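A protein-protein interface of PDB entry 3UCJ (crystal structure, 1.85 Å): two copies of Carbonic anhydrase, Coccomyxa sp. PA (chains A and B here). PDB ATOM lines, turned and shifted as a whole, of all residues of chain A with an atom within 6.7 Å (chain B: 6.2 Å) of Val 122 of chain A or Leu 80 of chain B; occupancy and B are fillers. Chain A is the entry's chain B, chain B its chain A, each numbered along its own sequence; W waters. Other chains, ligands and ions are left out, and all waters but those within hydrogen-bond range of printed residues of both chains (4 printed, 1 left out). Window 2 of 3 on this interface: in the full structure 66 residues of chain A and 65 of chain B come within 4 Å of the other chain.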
ATOM      1  N   ASP A  79      -5.915  -0.353   4.027  1.00  0.00           N
ATOM      2  CA  ASP A  79      -6.186   0.935   3.297  1.00  0.00           C
ATOM      3  C   ASP A  79      -5.373   2.057   3.933  1.00  0.00           C
ATOM      4  O   ASP A  79      -5.737   2.594   4.970  1.00  0.00           O
ATOM      5  CB  ASP A  79      -7.684   1.239   3.473  1.00  0.00           C
ATOM      6  CG  ASP A  79      -8.080   2.638   2.853  1.00  0.00           C
ATOM      7  OD1 ASP A  79      -7.267   3.099   2.041  1.00  0.00           O
ATOM      8  OD2 ASP A  79      -9.097   3.236   3.271  1.00  0.00           O
ATOM      9  N   ASN A  81      -5.300   5.002   2.941  1.00  0.00           N
ATOM     10  CA  ASN A  81      -6.090   6.205   3.015  1.00  0.00           C
ATOM     11  C   ASN A  81      -6.787   6.343   4.368  1.00  0.00           C
ATOM     12  O   ASN A  81      -6.562   7.386   5.062  1.00  0.00           O
ATOM     13  CB  ASN A  81      -7.089   6.197   1.782  1.00  0.00           C
ATOM     14  CG  ASN A  81      -7.970   7.437   1.748  1.00  0.00           C
ATOM     15  OD1 ASN A  81      -8.296   8.092   2.798  1.00  0.00           O
ATOM     16  ND2 ASN A  81      -8.371   7.793   0.479  1.00  0.00           N
ATOM     17  N   THR A 119     -19.263  -8.408 -10.882  1.00  0.00           N
ATOM     18  CA  THR A 119     -19.612  -7.043 -11.383  1.00  0.00           C
ATOM     19  C   THR A 119     -18.316  -6.223 -11.620  1.00  0.00           C
ATOM     20  O   THR A 119     -17.381  -6.289 -10.759  1.00  0.00           O
ATOM     21  CB  THR A 119     -20.470  -6.327 -10.416  1.00  0.00           C
ATOM     22  OG1 THR A 119     -21.689  -7.056 -10.197  1.00  0.00           O
ATOM     23  CG2 THR A 119     -20.762  -4.883 -10.839  1.00  0.00           C
ATOM     24  N   ALA A 120     -18.203  -5.522 -12.768  1.00  0.00           N
ATOM     25  CA  ALA A 120     -16.935  -4.855 -13.129  1.00  0.00           C
ATOM     26  C   ALA A 120     -16.770  -3.585 -12.253  1.00  0.00           C
ATOM     27  O   ALA A 120     -17.764  -3.030 -11.780  1.00  0.00           O
ATOM     28  CB  ALA A 120     -16.921  -4.413 -14.590  1.00  0.00           C
ATOM     29  N   GLY A 121     -15.529  -3.098 -12.202  1.00  0.00           N
ATOM     30  CA  GLY A 121     -15.300  -1.727 -11.685  1.00  0.00           C
ATOM     31  C   GLY A 121     -14.703  -1.709 -10.271  1.00  0.00           C
ATOM     32  O   GLY A 121     -14.776  -2.686  -9.512  1.00  0.00           O
ATOM     33  N   VAL A 122     -14.118  -0.560  -9.901  1.00  0.00           N
ATOM     34  CA  VAL A 122     -13.471  -0.501  -8.604  1.00  0.00           C
ATOM     35  C   VAL A 122     -14.461  -0.483  -7.433  1.00  0.00           C
ATOM     36  O   VAL A 122     -14.073  -0.937  -6.370  1.00  0.00           O
ATOM     37  CB  VAL A 122     -12.566   0.753  -8.487  1.00  0.00           C
ATOM     38  CG1 VAL A 122     -11.390   0.634  -9.459  1.00  0.00           C
ATOM     39  CG2 VAL A 122     -13.390   2.002  -8.762  1.00  0.00           C
ATOM     40  N   THR A 123     -15.660   0.109  -7.525  1.00  0.00           N
ATOM     41  CA  THR A 123     -16.605   0.080  -6.398  1.00  0.00           C
ATOM     42  C   THR A 123     -16.877  -1.348  -5.965  1.00  0.00           C
ATOM     43  O   THR A 123     -16.930  -1.634  -4.752  1.00  0.00           O
ATOM     44  CB  THR A 123     -17.930   0.824  -6.714  1.00  0.00           C
ATOM     45  OG1 THR A 123     -17.575   2.146  -7.144  1.00  0.00           O
ATOM     46  CG2 THR A 123     -18.706   0.988  -5.467  1.00  0.00           C
ATOM     47  N   ASN A 124     -17.037  -2.255  -6.908  1.00  0.00           N
ATOM     48  CA  ASN A 124     -17.353  -3.640  -6.480  1.00  0.00           C
ATOM     49  C   ASN A 124     -16.164  -4.197  -5.716  1.00  0.00           C
ATOM     50  O   ASN A 124     -16.327  -5.064  -4.799  1.00  0.00           O
ATOM     51  CB  ASN A 124     -17.502  -4.497  -7.779  1.00  0.00           C
ATOM     52  CG  ASN A 124     -17.774  -5.947  -7.442  1.00  0.00           C
ATOM     53  OD1 ASN A 124     -18.730  -6.217  -6.683  1.00  0.00           O
ATOM     54  ND2 ASN A 124     -16.847  -6.830  -7.801  1.00  0.00           N
ATOM     55  N   LEU A 125     -14.942  -3.820  -6.151  1.00  0.00           N
ATOM     56  CA  LEU A 125     -13.720  -4.306  -5.353  1.00  0.00           C
ATOM     57  C   LEU A 125     -13.848  -3.741  -3.940  1.00  0.00           C
ATOM     58  O   LEU A 125     -13.677  -4.500  -2.946  1.00  0.00           O
ATOM     59  CB  LEU A 125     -12.400  -3.838  -6.004  1.00  0.00           C
ATOM     60  CG  LEU A 125     -12.183  -4.236  -7.439  1.00  0.00           C
ATOM     61  CD1 LEU A 125     -10.861  -3.755  -8.033  1.00  0.00           C
ATOM     62  CD2 LEU A 125     -12.286  -5.804  -7.597  1.00  0.00           C
ATOM     63  N   TRP A 126     -14.067  -2.410  -3.884  1.00  0.00           N
ATOM     64  CA  TRP A 126     -14.074  -1.704  -2.605  1.00  0.00           C
ATOM     65  C   TRP A 126     -15.091  -2.209  -1.595  1.00  0.00           C
ATOM     66  O   TRP A 126     -14.781  -2.363  -0.388  1.00  0.00           O
ATOM     67  CB  TRP A 126     -14.272  -0.179  -2.848  1.00  0.00           C
ATOM     68  CG  TRP A 126     -14.361   0.611  -1.591  1.00  0.00           C
ATOM     69  CD1 TRP A 126     -15.460   1.082  -0.945  1.00  0.00           C
ATOM     70  CD2 TRP A 126     -13.245   0.995  -0.830  1.00  0.00           C
ATOM     71  NE1 TRP A 126     -15.080   1.771   0.201  1.00  0.00           N
ATOM     72  CE2 TRP A 126     -13.720   1.711   0.297  1.00  0.00           C
ATOM     73  CE3 TRP A 126     -11.860   0.766  -0.982  1.00  0.00           C
ATOM     74  CZ2 TRP A 126     -12.870   2.202   1.280  1.00  0.00           C
ATOM     75  CZ3 TRP A 126     -11.004   1.280   0.074  1.00  0.00           C
ATOM     76  CH2 TRP A 126     -11.528   1.972   1.113  1.00  0.00           C
ATOM     77  N   ILE A 127     -16.251  -2.682  -2.071  1.00  0.00           N
ATOM     78  CA  ILE A 127     -17.251  -3.134  -1.088  1.00  0.00           C
ATOM     79  C   ILE A 127     -17.072  -4.594  -0.726  1.00  0.00           C
ATOM     80  O   ILE A 127     -17.891  -5.143   0.011  1.00  0.00           O
ATOM     81  CB  ILE A 127     -18.675  -2.897  -1.591  1.00  0.00           C
ATOM     82  CG1 ILE A 127     -18.920  -3.698  -2.882  1.00  0.00           C
ATOM     83  CG2 ILE A 127     -18.902  -1.407  -1.794  1.00  0.00           C
ATOM     84  CD1 ILE A 127     -20.460  -3.513  -3.242  1.00  0.00           C
ATOM     85  N   SER B  76      -5.242   9.085  -6.546  1.00  0.00           N
ATOM     86  CA  SER B  76      -4.423   8.232  -7.300  1.00  0.00           C
ATOM     87  C   SER B  76      -5.321   7.138  -7.917  1.00  0.00           C
ATOM     88  O   SER B  76      -6.216   6.647  -7.230  1.00  0.00           O
ATOM     89  CB  SER B  76      -3.492   7.453  -6.304  1.00  0.00           C
ATOM     90  OG  SER B  76      -2.811   6.418  -7.015  1.00  0.00           O
ATOM     91  N   ASN B  77      -4.962   6.699  -9.137  1.00  0.00           N
ATOM     92  CA  ASN B  77      -5.686   5.592  -9.829  1.00  0.00           C
ATOM     93  C   ASN B  77      -5.553   4.308  -9.057  1.00  0.00           C
ATOM     94  O   ASN B  77      -6.442   3.406  -9.143  1.00  0.00           O
ATOM     95  CB  ASN B  77      -5.031   5.336 -11.164  1.00  0.00           C
ATOM     96  CG  ASN B  77      -5.298   6.463 -12.225  1.00  0.00           C
ATOM     97  OD1 ASN B  77      -6.189   7.313 -12.080  1.00  0.00           O
ATOM     98  ND2 ASN B  77      -4.493   6.427 -13.264  1.00  0.00           N
ATOM     99  N   LYS B  78      -4.506   4.267  -8.196  1.00  0.00           N
ATOM    100  CA  LYS B  78      -4.304   3.036  -7.426  1.00  0.00           C
ATOM    101  C   LYS B  78      -4.836   3.085  -6.040  1.00  0.00           C
ATOM    102  O   LYS B  78      -4.540   2.183  -5.252  1.00  0.00           O
ATOM    103  CB  LYS B  78      -2.826   2.676  -7.499  1.00  0.00           C
ATOM    104  CG  LYS B  78      -2.463   2.274  -8.945  1.00  0.00           C
ATOM    105  CD  LYS B  78      -0.971   2.126  -9.277  1.00  0.00           C
ATOM    106  CE  LYS B  78      -0.320   0.872  -8.514  1.00  0.00           C
ATOM    107  NZ  LYS B  78       1.008   0.442  -9.172  1.00  0.00           N
ATOM    108  N   ASP B  79      -5.642   4.084  -5.695  1.00  0.00           N
ATOM    109  CA  ASP B  79      -6.285   4.137  -4.412  1.00  0.00           C
ATOM    110  C   ASP B  79      -7.761   3.853  -4.614  1.00  0.00           C
ATOM    111  O   ASP B  79      -8.474   4.791  -5.077  1.00  0.00           O
ATOM    112  CB  ASP B  79      -6.213   5.591  -3.843  1.00  0.00           C
ATOM    113  CG  ASP B  79      -7.108   5.775  -2.604  1.00  0.00           C
ATOM    114  OD1 ASP B  79      -7.395   4.768  -1.910  1.00  0.00           O
ATOM    115  OD2 ASP B  79      -7.374   6.953  -2.235  1.00  0.00           O
ATOM    116  N   LEU B  80      -8.138   2.601  -4.268  1.00  0.00           N
ATOM    117  CA  LEU B  80      -9.544   2.154  -4.381  1.00  0.00           C
ATOM    118  C   LEU B  80     -10.526   2.951  -3.547  1.00  0.00           C
ATOM    119  O   LEU B  80     -11.719   2.982  -3.842  1.00  0.00           O
ATOM    120  CB  LEU B  80      -9.692   0.649  -4.153  1.00  0.00           C
ATOM    121  CG  LEU B  80      -8.865  -0.191  -5.124  1.00  0.00           C
ATOM    122  CD1 LEU B  80      -9.070  -1.738  -4.709  1.00  0.00           C
ATOM    123  CD2 LEU B  80      -9.327   0.101  -6.624  1.00  0.00           C
ATOM    124  N   ASN B  81     -10.086   3.576  -2.445  1.00  0.00           N
ATOM    125  CA  ASN B  81     -10.945   4.390  -1.643  1.00  0.00           C
ATOM    126  C   ASN B  81     -11.390   5.657  -2.429  1.00  0.00           C
ATOM    127  O   ASN B  81     -12.604   5.917  -2.673  1.00  0.00           O
ATOM    128  CB  ASN B  81     -10.119   4.809  -0.337  1.00  0.00           C
ATOM    129  CG  ASN B  81     -10.909   5.586   0.664  1.00  0.00           C
ATOM    130  OD1 ASN B  81     -11.658   6.526   0.334  1.00  0.00           O
ATOM    131  ND2 ASN B  81     -10.588   5.342   1.996  1.00  0.00           N
ATOM    132  N   CYS B  82     -10.426   6.511  -2.791  1.00  0.00           N
ATOM    133  CA  CYS B  82     -10.824   7.671  -3.620  1.00  0.00           C
ATOM    134  C   CYS B  82     -11.441   7.246  -4.988  1.00  0.00           C
ATOM    135  O   CYS B  82     -12.490   7.855  -5.447  1.00  0.00           O
ATOM    136  CB  CYS B  82      -9.565   8.495  -3.951  1.00  0.00           C
ATOM    137  SG  CYS B  82      -9.975  10.085  -4.798  1.00  0.00           S
ATOM    138  N   MET B  83     -10.884   6.226  -5.607  1.00  0.00           N
ATOM    139  CA  MET B  83     -11.408   5.810  -6.962  1.00  0.00           C
ATOM    140  C   MET B  83     -12.867   5.310  -6.899  1.00  0.00           C
ATOM    141  O   MET B  83     -13.658   5.591  -7.870  1.00  0.00           O
ATOM    142  CB  MET B  83     -10.511   4.787  -7.608  1.00  0.00           C
ATOM    143  CG  MET B  83      -9.145   5.402  -8.065  1.00  0.00           C
ATOM    144  SD  MET B  83      -9.460   6.513  -9.490  1.00  0.00           S
ATOM    145  CE  MET B  83      -8.998   8.085  -8.797  1.00  0.00           C
ATOM    146  N   SER B  84     -13.293   4.665  -5.804  1.00  0.00           N
ATOM    147  CA  SER B  84     -14.712   4.228  -5.612  1.00  0.00           C
ATOM    148  C   SER B  84     -15.678   5.409  -5.479  1.00  0.00           C
ATOM    149  O   SER B  84     -16.761   5.426  -6.052  1.00  0.00           O
ATOM    150  CB  SER B  84     -14.825   3.334  -4.344  1.00  0.00           C
ATOM    151  OG  SER B  84     -14.328   2.139  -4.821  1.00  0.00           O
ATOM    152  N   CYS B  85     -15.266   6.466  -4.800  1.00  0.00           N
ATOM    153  CA  CYS B  85     -16.061   7.668  -4.704  1.00  0.00           C
ATOM    154  C   CYS B  85     -16.173   8.309  -6.082  1.00  0.00           C
ATOM    155  O   CYS B  85     -17.311   8.784  -6.461  1.00  0.00           O
ATOM    156  CB  CYS B  85     -15.370   8.722  -3.824  1.00  0.00           C
ATOM    157  SG  CYS B  85     -15.432   8.306  -2.042  1.00  0.00           S
ATOM    158  N   GLU B  87     -15.823   6.708  -9.062  1.00  0.00           N
ATOM    159  CA  GLU B  87     -16.578   5.814  -9.985  1.00  0.00           C
ATOM    160  C   GLU B  87     -18.092   5.852  -9.642  1.00  0.00           C
ATOM    161  O   GLU B  87     -18.944   6.066 -10.562  1.00  0.00           O
ATOM    162  CB  GLU B  87     -16.131   4.365  -9.837  1.00  0.00           C
ATOM    163  CG  GLU B  87     -16.850   3.447 -10.812  1.00  0.00           C
ATOM    164  CD  GLU B  87     -16.373   1.990 -10.681  1.00  0.00           C
ATOM    165  OE1 GLU B  87     -16.915   1.341  -9.794  1.00  0.00           O
ATOM    166  OE2 GLU B  87     -15.581   1.475 -11.494  1.00  0.00           O
ATOM    167  N   ILE B 170     -11.926   6.829 -14.979  1.00  0.00           N
ATOM    168  CA  ILE B 170     -13.330   7.090 -14.751  1.00  0.00           C
ATOM    169  C   ILE B 170     -13.697   8.366 -15.534  1.00  0.00           C
ATOM    170  O   ILE B 170     -14.680   8.359 -16.265  1.00  0.00           O
ATOM    171  CB  ILE B 170     -13.648   7.362 -13.242  1.00  0.00           C
ATOM    172  CG1 ILE B 170     -13.331   6.119 -12.306  1.00  0.00           C
ATOM    173  CG2 ILE B 170     -15.100   7.898 -13.085  1.00  0.00           C
ATOM    174  CD1 ILE B 170     -13.666   4.810 -12.858  1.00  0.00           C
HETATM  175  O   HOH W   1      -6.340   2.814  -0.422  1.00  0.00           O
HETATM  176  O   HOH W   2     -20.015   2.440  -8.755  1.00  0.00           O
HETATM  177  O   HOH W   3     -14.587   4.925  -1.142  1.00  0.00           O
HETATM  178  O   HOH W   4     -13.098   1.041 -12.731  1.00  0.00           O
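Water W1 lies within hydrogen-bond range of the side-chain carboxylate of Asp 79 of chain A (2.6 Å) and the side-chain carboxylate of Asp 79 of chain B (2.7 Å). Water W3 lies within hydrogen-bond range of the backbone carbonyl oxygen of Asn 81 of chain B (2.7 Å), the indole nitrogen of Trp 126 of chain A (3.5 Å) and the side-chain sulfur of Cys 85 of chain B (3.6 Å). Water W4 lies within hydrogen-bond range of the side-chain carboxylate of Glu 87 of chain B (2.8 Å) and the backbone NH of Val 122 of chain A (3.4 Å). Water W2 lies within hydrogen-bond range of the side-chain hydroxyl (OG1) of Thr 123 of chain A and the side-chain carboxylate (OE1) of Glu 87 of chain B.
Printed residues of chain A that touch a printed residue of chain B: Asp 79, Asn 81, Gly 121, Val 122, Thr 123 and Trp 126. Hydrophobic or aromatic side chains of chain A within 4 Å of the printed part of chain B: Val 122 and Trp 126. Among the printed residues, no Asp or Glu carboxylate lies within 4 Å of a Lys or Arg side-chain nitrogen of the other chain.
Asn 81 of chain B touches Asn 81 of chain A (ND2 to CG, 3.4 Å). Glu 87 of chain B touches Gly 121 of chain A (OE2 to CA, 3.2 Å). CG1 of Val 122 of chain A touches CD2 of Leu 80 of chain B, 3.5 Å away. Met 83 of chain B touches Val 122 of chain A (O to CG2, 3.7 Å). Ser 84 of chain B touches Thr 123 of chain A (OG to CA, 3.5 Å). Trp 126 of chain A touches Leu 80 of chain B. Asn 81 of chain B touches Trp 126 of chain A. OG of Ser 84 of chain B touches CB of Trp 126 of chain A (3.0 Å).
Asp 79 of chain A touches Asn 81 of chain B, and with the chains exchanged Asn 81 of chain A touches Asp 79 of chain B. Asn 81 of chain B touches its own counterpart, Asn 81 of chain A.
OD2 of Asp 79 of chain B sits at hydrogen-bond distance from N of Cys 82 of chain B, at 3.1 Å. The backbone carbonyl oxygen (O) of Asn 81 of chain B is in hydrogen-bond range of the side-chain sulfur (SG) of Cys 85 of chain B. O of Leu 80 of chain B sits at hydrogen-bond distance from OG of Ser 84 of chain B (2.9 Å). The side-chain carboxylate (OD1) of Asp 79 of chain B is in hydrogen-bond range of the backbone NH (N) of Asn 81 of chain B (3.0 Å). The side-chain carboxylate (OD1) of Asp 79 of chain A sits at hydrogen-bond distance from the backbone NH (N) of Asn 81 of chain A.
The side-chain amide nitrogen (ND2) of Asn 81 of chain A lies within hydrogen-bond range of the side-chain carboxylate (OD2) of Asp 79 of chain B. The side-chain carboxylate (OE2) of Glu 87 of chain B is in hydrogen-bond range of the backbone NH (N) of Val 122 of chain A, at 3.0 Å. The side-chain hydroxyl (OG1) of Thr 123 of chain A lies within hydrogen-bond range of the side-chain carboxylate (OE1) of Glu 87 of chain B (2.8 Å). The side-chain carboxylate (OD2) of Asp 79 of chain A sits at hydrogen-bond distance from the side-chain amide nitrogen (ND2) of Asn 81 of chain B, 2.9 Å away. The side-chain hydroxyl (OG) of Ser 84 of chain B lies within hydrogen-bond range of the backbone carbonyl oxygen (O) of Val 122 of chain A (3.5 Å).
Val 122 of chain A touches just these residues of chain B: Leu 80 (3.5 Å), Met 83 (3.7 Å), Ser 84 (3.5 Å) and Glu 87 (3.0 Å). Leu 80 of chain B touches two residues of chain A. Of the printed residues of chain B, Gly 121 of chain A touches Glu 87. Printed residues of chain A within 4 Å of Asp 79 of chain B: Asn 81. Leu 125 of chain A touches none of the printed residues of chain B. The nearest residue of chain A that does not touch Leu 80 of chain B is Leu 125 of chain A (4.1 Å).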
